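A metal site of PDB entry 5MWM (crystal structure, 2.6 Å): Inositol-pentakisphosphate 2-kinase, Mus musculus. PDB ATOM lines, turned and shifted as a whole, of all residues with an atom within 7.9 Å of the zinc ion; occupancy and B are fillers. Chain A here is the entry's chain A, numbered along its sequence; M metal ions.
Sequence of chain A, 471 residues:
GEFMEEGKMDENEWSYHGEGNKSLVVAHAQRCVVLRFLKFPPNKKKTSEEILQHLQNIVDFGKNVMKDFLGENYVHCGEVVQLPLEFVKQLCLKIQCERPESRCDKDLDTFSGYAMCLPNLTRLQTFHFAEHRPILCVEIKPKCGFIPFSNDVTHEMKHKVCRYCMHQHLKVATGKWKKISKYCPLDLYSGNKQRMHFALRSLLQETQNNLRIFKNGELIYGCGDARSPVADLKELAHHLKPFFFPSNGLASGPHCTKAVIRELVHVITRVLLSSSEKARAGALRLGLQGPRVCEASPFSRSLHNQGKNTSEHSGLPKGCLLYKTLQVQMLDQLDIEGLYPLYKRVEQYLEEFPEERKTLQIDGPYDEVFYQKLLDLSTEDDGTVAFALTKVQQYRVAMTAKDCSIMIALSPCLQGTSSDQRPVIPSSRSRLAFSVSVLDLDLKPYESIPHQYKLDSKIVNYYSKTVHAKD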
ATOM      1  N   CYS A 144      23.637  -8.804 -23.398  1.00  0.00           N
ATOM      2  CA  CYS A 144      22.831  -7.566 -23.454  1.00  0.00           C
ATOM      3  C   CYS A 144      21.460  -7.694 -22.795  1.00  0.00           C
ATOM      4  O   CYS A 144      20.720  -8.618 -23.080  1.00  0.00           O
ATOM      5  CB  CYS A 144      22.611  -7.081 -24.875  1.00  0.00           C
ATOM      6  SG  CYS A 144      21.880  -5.423 -24.835  1.00  0.00           S
ATOM      7  N   ILE A 147      16.215  -5.009 -25.429  1.00  0.00           N
ATOM      8  CA  ILE A 147      15.879  -5.150 -26.839  1.00  0.00           C
ATOM      9  C   ILE A 147      15.806  -3.754 -27.478  1.00  0.00           C
ATOM     10  O   ILE A 147      15.193  -2.844 -26.908  1.00  0.00           O
ATOM     11  CB  ILE A 147      14.538  -5.906 -27.021  1.00  0.00           C
ATOM     12  CG1 ILE A 147      14.615  -7.269 -26.317  1.00  0.00           C
ATOM     13  CG2 ILE A 147      14.224  -6.123 -28.496  1.00  0.00           C
ATOM     14  CD1 ILE A 147      13.382  -8.137 -26.490  1.00  0.00           C
ATOM     15  N   LYS A 160      11.257  -7.429 -31.068  1.00  0.00           N
ATOM     16  CA  LYS A 160      10.537  -8.457 -30.306  1.00  0.00           C
ATOM     17  C   LYS A 160      11.453  -9.452 -29.591  1.00  0.00           C
ATOM     18  O   LYS A 160      11.169  -9.871 -28.471  1.00  0.00           O
ATOM     19  CB  LYS A 160       9.589  -9.215 -31.234  1.00  0.00           C
ATOM     20  CG  LYS A 160       8.431  -8.383 -31.752  1.00  0.00           C
ATOM     21  CD  LYS A 160       7.786  -9.022 -32.972  1.00  0.00           C
ATOM     22  CE  LYS A 160       6.432  -8.419 -33.296  1.00  0.00           C
ATOM     23  NZ  LYS A 160       5.721  -9.208 -34.332  1.00  0.00           N
ATOM     24  N   VAL A 161      12.547  -9.842 -30.257  1.00  0.00           N
ATOM     25  CA  VAL A 161      13.514 -10.786 -29.702  1.00  0.00           C
ATOM     26  C   VAL A 161      14.856 -10.112 -29.389  1.00  0.00           C
ATOM     27  O   VAL A 161      15.327  -9.246 -30.140  1.00  0.00           O
ATOM     28  CB  VAL A 161      13.740 -11.963 -30.672  1.00  0.00           C
ATOM     29  CG1 VAL A 161      14.455 -13.113 -29.979  1.00  0.00           C
ATOM     30  CG2 VAL A 161      12.407 -12.439 -31.244  1.00  0.00           C
ATOM     31  N   CYS A 162      15.474 -10.509 -28.281  1.00  0.00           N
ATOM     32  CA  CYS A 162      16.776  -9.965 -27.887  1.00  0.00           C
ATOM     33  C   CYS A 162      17.872 -10.552 -28.758  1.00  0.00           C
ATOM     34  O   CYS A 162      17.694 -11.598 -29.373  1.00  0.00           O
ATOM     35  CB  CYS A 162      17.063 -10.308 -26.436  1.00  0.00           C
ATOM     36  SG  CYS A 162      17.297 -12.076 -26.153  1.00  0.00           S
ATOM     37  N   ARG A 163      19.006  -9.843 -28.790  1.00  0.00           N
ATOM     38  CA  ARG A 163      20.199 -10.262 -29.555  1.00  0.00           C
ATOM     39  C   ARG A 163      20.639 -11.681 -29.210  1.00  0.00           C
ATOM     40  O   ARG A 163      20.812 -12.530 -30.104  1.00  0.00           O
ATOM     41  CB  ARG A 163      21.348  -9.266 -29.307  1.00  0.00           C
ATOM     42  CG  ARG A 163      22.765  -9.722 -29.658  1.00  0.00           C
ATOM     43  CD  ARG A 163      22.950 -10.121 -31.117  1.00  0.00           C
ATOM     44  NE  ARG A 163      24.376 -10.030 -31.450  1.00  0.00           N
ATOM     45  CZ  ARG A 163      24.988  -9.030 -32.109  1.00  0.00           C
ATOM     46  NH1 ARG A 163      24.314  -7.993 -32.600  1.00  0.00           N
ATOM     47  NH2 ARG A 163      26.307  -9.100 -32.296  1.00  0.00           N
ATOM     48  N   TYR A 164      20.808 -11.922 -27.918  1.00  0.00           N
ATOM     49  CA  TYR A 164      21.251 -13.221 -27.409  1.00  0.00           C
ATOM     50  C   TYR A 164      20.443 -14.405 -27.980  1.00  0.00           C
ATOM     51  O   TYR A 164      21.024 -15.342 -28.549  1.00  0.00           O
ATOM     52  CB  TYR A 164      21.157 -13.249 -25.888  1.00  0.00           C
ATOM     53  CG  TYR A 164      21.700 -14.511 -25.309  1.00  0.00           C
ATOM     54  CD1 TYR A 164      20.882 -15.621 -25.111  1.00  0.00           C
ATOM     55  CD2 TYR A 164      23.045 -14.605 -24.967  1.00  0.00           C
ATOM     56  CE1 TYR A 164      21.398 -16.797 -24.582  1.00  0.00           C
ATOM     57  CE2 TYR A 164      23.578 -15.767 -24.431  1.00  0.00           C
ATOM     58  CZ  TYR A 164      22.754 -16.863 -24.246  1.00  0.00           C
ATOM     59  OH  TYR A 164      23.294 -18.016 -23.703  1.00  0.00           O
ATOM     60  N   CYS A 165      19.125 -14.340 -27.814  1.00  0.00           N
ATOM     61  CA  CYS A 165      18.210 -15.429 -28.224  1.00  0.00           C
ATOM     62  C   CYS A 165      18.224 -15.696 -29.733  1.00  0.00           C
ATOM     63  O   CYS A 165      18.199 -16.866 -30.139  1.00  0.00           O
ATOM     64  CB  CYS A 165      16.775 -15.145 -27.738  1.00  0.00           C
ATOM     65  SG  CYS A 165      16.518 -15.360 -25.960  1.00  0.00           S
ATOM     66  N   MET A 166      18.275 -14.644 -30.551  1.00  0.00           N
ATOM     67  CA  MET A 166      18.440 -14.816 -32.001  1.00  0.00           C
ATOM     68  C   MET A 166      19.764 -15.499 -32.320  1.00  0.00           C
ATOM     69  O   MET A 166      19.778 -16.441 -33.108  1.00  0.00           O
ATOM     70  CB  MET A 166      18.473 -13.493 -32.728  1.00  0.00           C
ATOM     71  CG  MET A 166      17.206 -12.675 -32.635  1.00  0.00           C
ATOM     72  SD  MET A 166      17.127 -11.570 -34.055  1.00  0.00           S
ATOM     73  CE  MET A 166      16.708 -10.037 -33.254  1.00  0.00           C
ATOM     74  N   SER A 181      20.062 -22.532 -25.917  1.00  0.00           N
ATOM     75  CA  SER A 181      19.899 -22.174 -24.498  1.00  0.00           C
ATOM     76  C   SER A 181      18.547 -21.468 -24.282  1.00  0.00           C
ATOM     77  O   SER A 181      18.135 -20.605 -25.071  1.00  0.00           O
ATOM     78  CB  SER A 181      21.049 -21.289 -23.993  1.00  0.00           C
ATOM     79  OG  SER A 181      21.082 -21.222 -22.574  1.00  0.00           O
ATOM     80  N   LYS A 182      17.897 -21.832 -23.179  1.00  0.00           N
ATOM     81  CA  LYS A 182      16.611 -21.257 -22.779  1.00  0.00           C
ATOM     82  C   LYS A 182      16.785 -19.959 -21.991  1.00  0.00           C
ATOM     83  O   LYS A 182      15.809 -19.266 -21.697  1.00  0.00           O
ATOM     84  CB  LYS A 182      15.836 -22.255 -21.908  1.00  0.00           C
ATOM     85  CG  LYS A 182      15.653 -23.647 -22.494  1.00  0.00           C
ATOM     86  CD  LYS A 182      15.089 -24.588 -21.431  1.00  0.00           C
ATOM     87  CE  LYS A 182      15.427 -26.037 -21.732  1.00  0.00           C
ATOM     88  NZ  LYS A 182      14.785 -26.497 -22.991  1.00  0.00           N
ATOM     89  N   TYR A 183      18.029 -19.662 -21.605  1.00  0.00           N
ATOM     90  CA  TYR A 183      18.408 -18.370 -21.041  1.00  0.00           C
ATOM     91  C   TYR A 183      18.086 -17.220 -22.015  1.00  0.00           C
ATOM     92  O   TYR A 183      18.488 -17.267 -23.178  1.00  0.00           O
ATOM     93  CB  TYR A 183      19.900 -18.366 -20.680  1.00  0.00           C
ATOM     94  CG  TYR A 183      20.452 -17.026 -20.262  1.00  0.00           C
ATOM     95  CD1 TYR A 183      20.242 -16.525 -18.994  1.00  0.00           C
ATOM     96  CD2 TYR A 183      21.193 -16.251 -21.143  1.00  0.00           C
ATOM     97  CE1 TYR A 183      20.745 -15.290 -18.605  1.00  0.00           C
ATOM     98  CE2 TYR A 183      21.691 -15.008 -20.774  1.00  0.00           C
ATOM     99  CZ  TYR A 183      21.470 -14.535 -19.499  1.00  0.00           C
ATOM    100  OH  TYR A 183      21.973 -13.306 -19.132  1.00  0.00           O
ATOM    101  N   CYS A 184      17.331 -16.240 -21.530  1.00  0.00           N
ATOM    102  CA  CYS A 184      17.208 -14.943 -22.191  1.00  0.00           C
ATOM    103  C   CYS A 184      17.767 -13.933 -21.195  1.00  0.00           C
ATOM    104  O   CYS A 184      17.446 -14.010 -20.007  1.00  0.00           O
ATOM    105  CB  CYS A 184      15.738 -14.626 -22.506  1.00  0.00           C
ATOM    106  SG  CYS A 184      15.430 -12.936 -23.092  1.00  0.00           S
ATOM    107  N   PRO A 185      18.615 -12.997 -21.650  1.00  0.00           N
ATOM    108  CA  PRO A 185      19.152 -12.047 -20.677  1.00  0.00           C
ATOM    109  C   PRO A 185      18.109 -11.163 -19.993  1.00  0.00           C
ATOM    110  O   PRO A 185      18.338 -10.751 -18.860  1.00  0.00           O
ATOM    111  CB  PRO A 185      20.101 -11.186 -21.505  1.00  0.00           C
ATOM    112  CG  PRO A 185      20.467 -12.018 -22.670  1.00  0.00           C
ATOM    113  CD  PRO A 185      19.260 -12.871 -22.966  1.00  0.00           C
ATOM    114  N   LEU A 186      16.989 -10.868 -20.671  1.00  0.00           N
ATOM    115  CA  LEU A 186      15.929 -10.023 -20.101  1.00  0.00           C
ATOM    116  C   LEU A 186      15.268 -10.633 -18.856  1.00  0.00           C
ATOM    117  O   LEU A 186      14.782  -9.903 -17.997  1.00  0.00           O
ATOM    118  CB  LEU A 186      14.855  -9.682 -21.131  1.00  0.00           C
ATOM    119  CG  LEU A 186      15.210  -8.482 -22.004  1.00  0.00           C
ATOM    120  CD1 LEU A 186      16.317  -8.788 -22.994  1.00  0.00           C
ATOM    121  CD2 LEU A 186      13.961  -8.001 -22.740  1.00  0.00           C
ATOM    122  N   ASP A 187      15.252 -11.965 -18.780  1.00  0.00           N
ATOM    123  CA  ASP A 187      14.853 -12.649 -17.563  1.00  0.00           C
ATOM    124  C   ASP A 187      15.776 -12.225 -16.426  1.00  0.00           C
ATOM    125  O   ASP A 187      15.299 -11.808 -15.366  1.00  0.00           O
ATOM    126  CB  ASP A 187      14.911 -14.178 -17.730  1.00  0.00           C
ATOM    127  CG  ASP A 187      13.852 -14.738 -18.696  1.00  0.00           C
ATOM    128  OD1 ASP A 187      12.780 -14.112 -18.902  1.00  0.00           O
ATOM    129  OD2 ASP A 187      14.107 -15.835 -19.258  1.00  0.00           O
ATOM    130  N   ARG A 195      11.746 -14.937 -12.541  1.00  0.00           N
ATOM    131  CA  ARG A 195      12.437 -14.872 -13.838  1.00  0.00           C
ATOM    132  C   ARG A 195      13.938 -15.055 -13.676  1.00  0.00           C
ATOM    133  O   ARG A 195      14.551 -15.835 -14.403  1.00  0.00           O
ATOM    134  CB  ARG A 195      12.183 -13.521 -14.530  1.00  0.00           C
ATOM    135  CG  ARG A 195      10.786 -13.377 -15.106  1.00  0.00           C
ATOM    136  CD  ARG A 195      10.609 -12.035 -15.815  1.00  0.00           C
ATOM    137  NE  ARG A 195      11.169 -12.034 -17.164  1.00  0.00           N
ATOM    138  CZ  ARG A 195      11.241 -10.976 -17.970  1.00  0.00           C
ATOM    139  NH1 ARG A 195      10.797  -9.788 -17.573  1.00  0.00           N
ATOM    140  NH2 ARG A 195      11.764 -11.101 -19.188  1.00  0.00           N
ATOM    141  N   VAL A 293      10.095  -7.663 -21.859  1.00  0.00           N
ATOM    142  CA  VAL A 293       9.965  -9.118 -22.020  1.00  0.00           C
ATOM    143  C   VAL A 293      10.245  -9.536 -23.470  1.00  0.00           C
ATOM    144  O   VAL A 293       9.690  -8.958 -24.424  1.00  0.00           O
ATOM    145  CB  VAL A 293       8.562  -9.618 -21.601  1.00  0.00           C
ATOM    146  CG1 VAL A 293       8.429 -11.131 -21.794  1.00  0.00           C
ATOM    147  CG2 VAL A 293       8.277  -9.241 -20.146  1.00  0.00           C
ATOM    148  N   CYS A 294      11.103 -10.537 -23.619  1.00  0.00           N
ATOM    149  CA  CYS A 294      11.471 -11.096 -24.924  1.00  0.00           C
ATOM    150  C   CYS A 294      10.452 -12.138 -25.354  1.00  0.00           C
ATOM    151  O   CYS A 294       9.920 -12.883 -24.532  1.00  0.00           O
ATOM    152  CB  CYS A 294      12.841 -11.750 -24.854  1.00  0.00           C
ATOM    153  SG  CYS A 294      13.312 -12.581 -26.388  1.00  0.00           S
ATOM    154  N   GLU A 295      10.213 -12.201 -26.664  1.00  0.00           N
ATOM    155  CA  GLU A 295       9.232 -13.119 -27.212  1.00  0.00           C
ATOM    156  C   GLU A 295       9.729 -14.561 -27.161  1.00  0.00           C
ATOM    157  O   GLU A 295       8.938 -15.476 -26.918  1.00  0.00           O
ATOM    158  CB  GLU A 295       8.901 -12.717 -28.653  1.00  0.00           C
ATOM    159  CG  GLU A 295       7.634 -13.337 -29.214  1.00  0.00           C
ATOM    160  CD  GLU A 295       7.198 -12.673 -30.498  1.00  0.00           C
ATOM    161  OE1 GLU A 295       7.108 -13.370 -31.530  1.00  0.00           O
ATOM    162  OE2 GLU A 295       6.963 -11.451 -30.487  1.00  0.00           O
ATOM    163  N   ALA A 296      11.023 -14.749 -27.388  1.00  0.00           N
ATOM    164  CA  ALA A 296      11.651 -16.081 -27.438  1.00  0.00           C
ATOM    165  C   ALA A 296      11.842 -16.760 -26.076  1.00  0.00           C
ATOM    166  O   ALA A 296      11.969 -17.990 -26.025  1.00  0.00           O
ATOM    167  CB  ALA A 296      12.978 -15.998 -28.174  1.00  0.00           C
ATOM    168  N   SER A 297      11.887 -15.986 -24.999  1.00  0.00           N
ATOM    169  CA  SER A 297      12.107 -16.517 -23.645  1.00  0.00           C
ATOM    170  C   SER A 297      11.021 -17.530 -23.296  1.00  0.00           C
ATOM    171  O   SER A 297       9.846 -17.170 -23.271  1.00  0.00           O
ATOM    172  CB  SER A 297      12.090 -15.391 -22.603  1.00  0.00           C
ATOM    173  OG  SER A 297      12.131 -15.909 -21.285  1.00  0.00           O
ATOM    174  N   PRO A 298      11.396 -18.803 -23.055  1.00  0.00           N
ATOM    175  CA  PRO A 298      10.397 -19.810 -22.666  1.00  0.00           C
ATOM    176  C   PRO A 298      10.213 -19.856 -21.149  1.00  0.00           C
ATOM    177  O   PRO A 298      10.942 -20.562 -20.458  1.00  0.00           O
ATOM    178  CB  PRO A 298      10.997 -21.106 -23.216  1.00  0.00           C
ATOM    179  CG  PRO A 298      12.472 -20.903 -23.148  1.00  0.00           C
ATOM    180  CD  PRO A 298      12.730 -19.411 -23.186  1.00  0.00           C
HETATM  181 ZN    ZN M   1      15.651 -13.286 -25.244  1.00  0.00          ZN
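The zinc ion is bound by SG of Cys 184 (2.2 Å), SG of Cys 162 (2.2 Å), SG of Cys 165 (2.4 Å) and SG of Cys 294 (2.7 Å).
The zinc ion has four donor atoms within binding distance.
Within 4 Å of the zinc ion: Cys 162, Cys 165, Cys 184 and Cys 294.
N of Leu 186 lies close to SG of Cys 184, 3.5 Å away.
The side-chain sulfur (SG) of Cys 294 sits close to the backbone NH (N) of Ala 296, 3.3 Å away.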
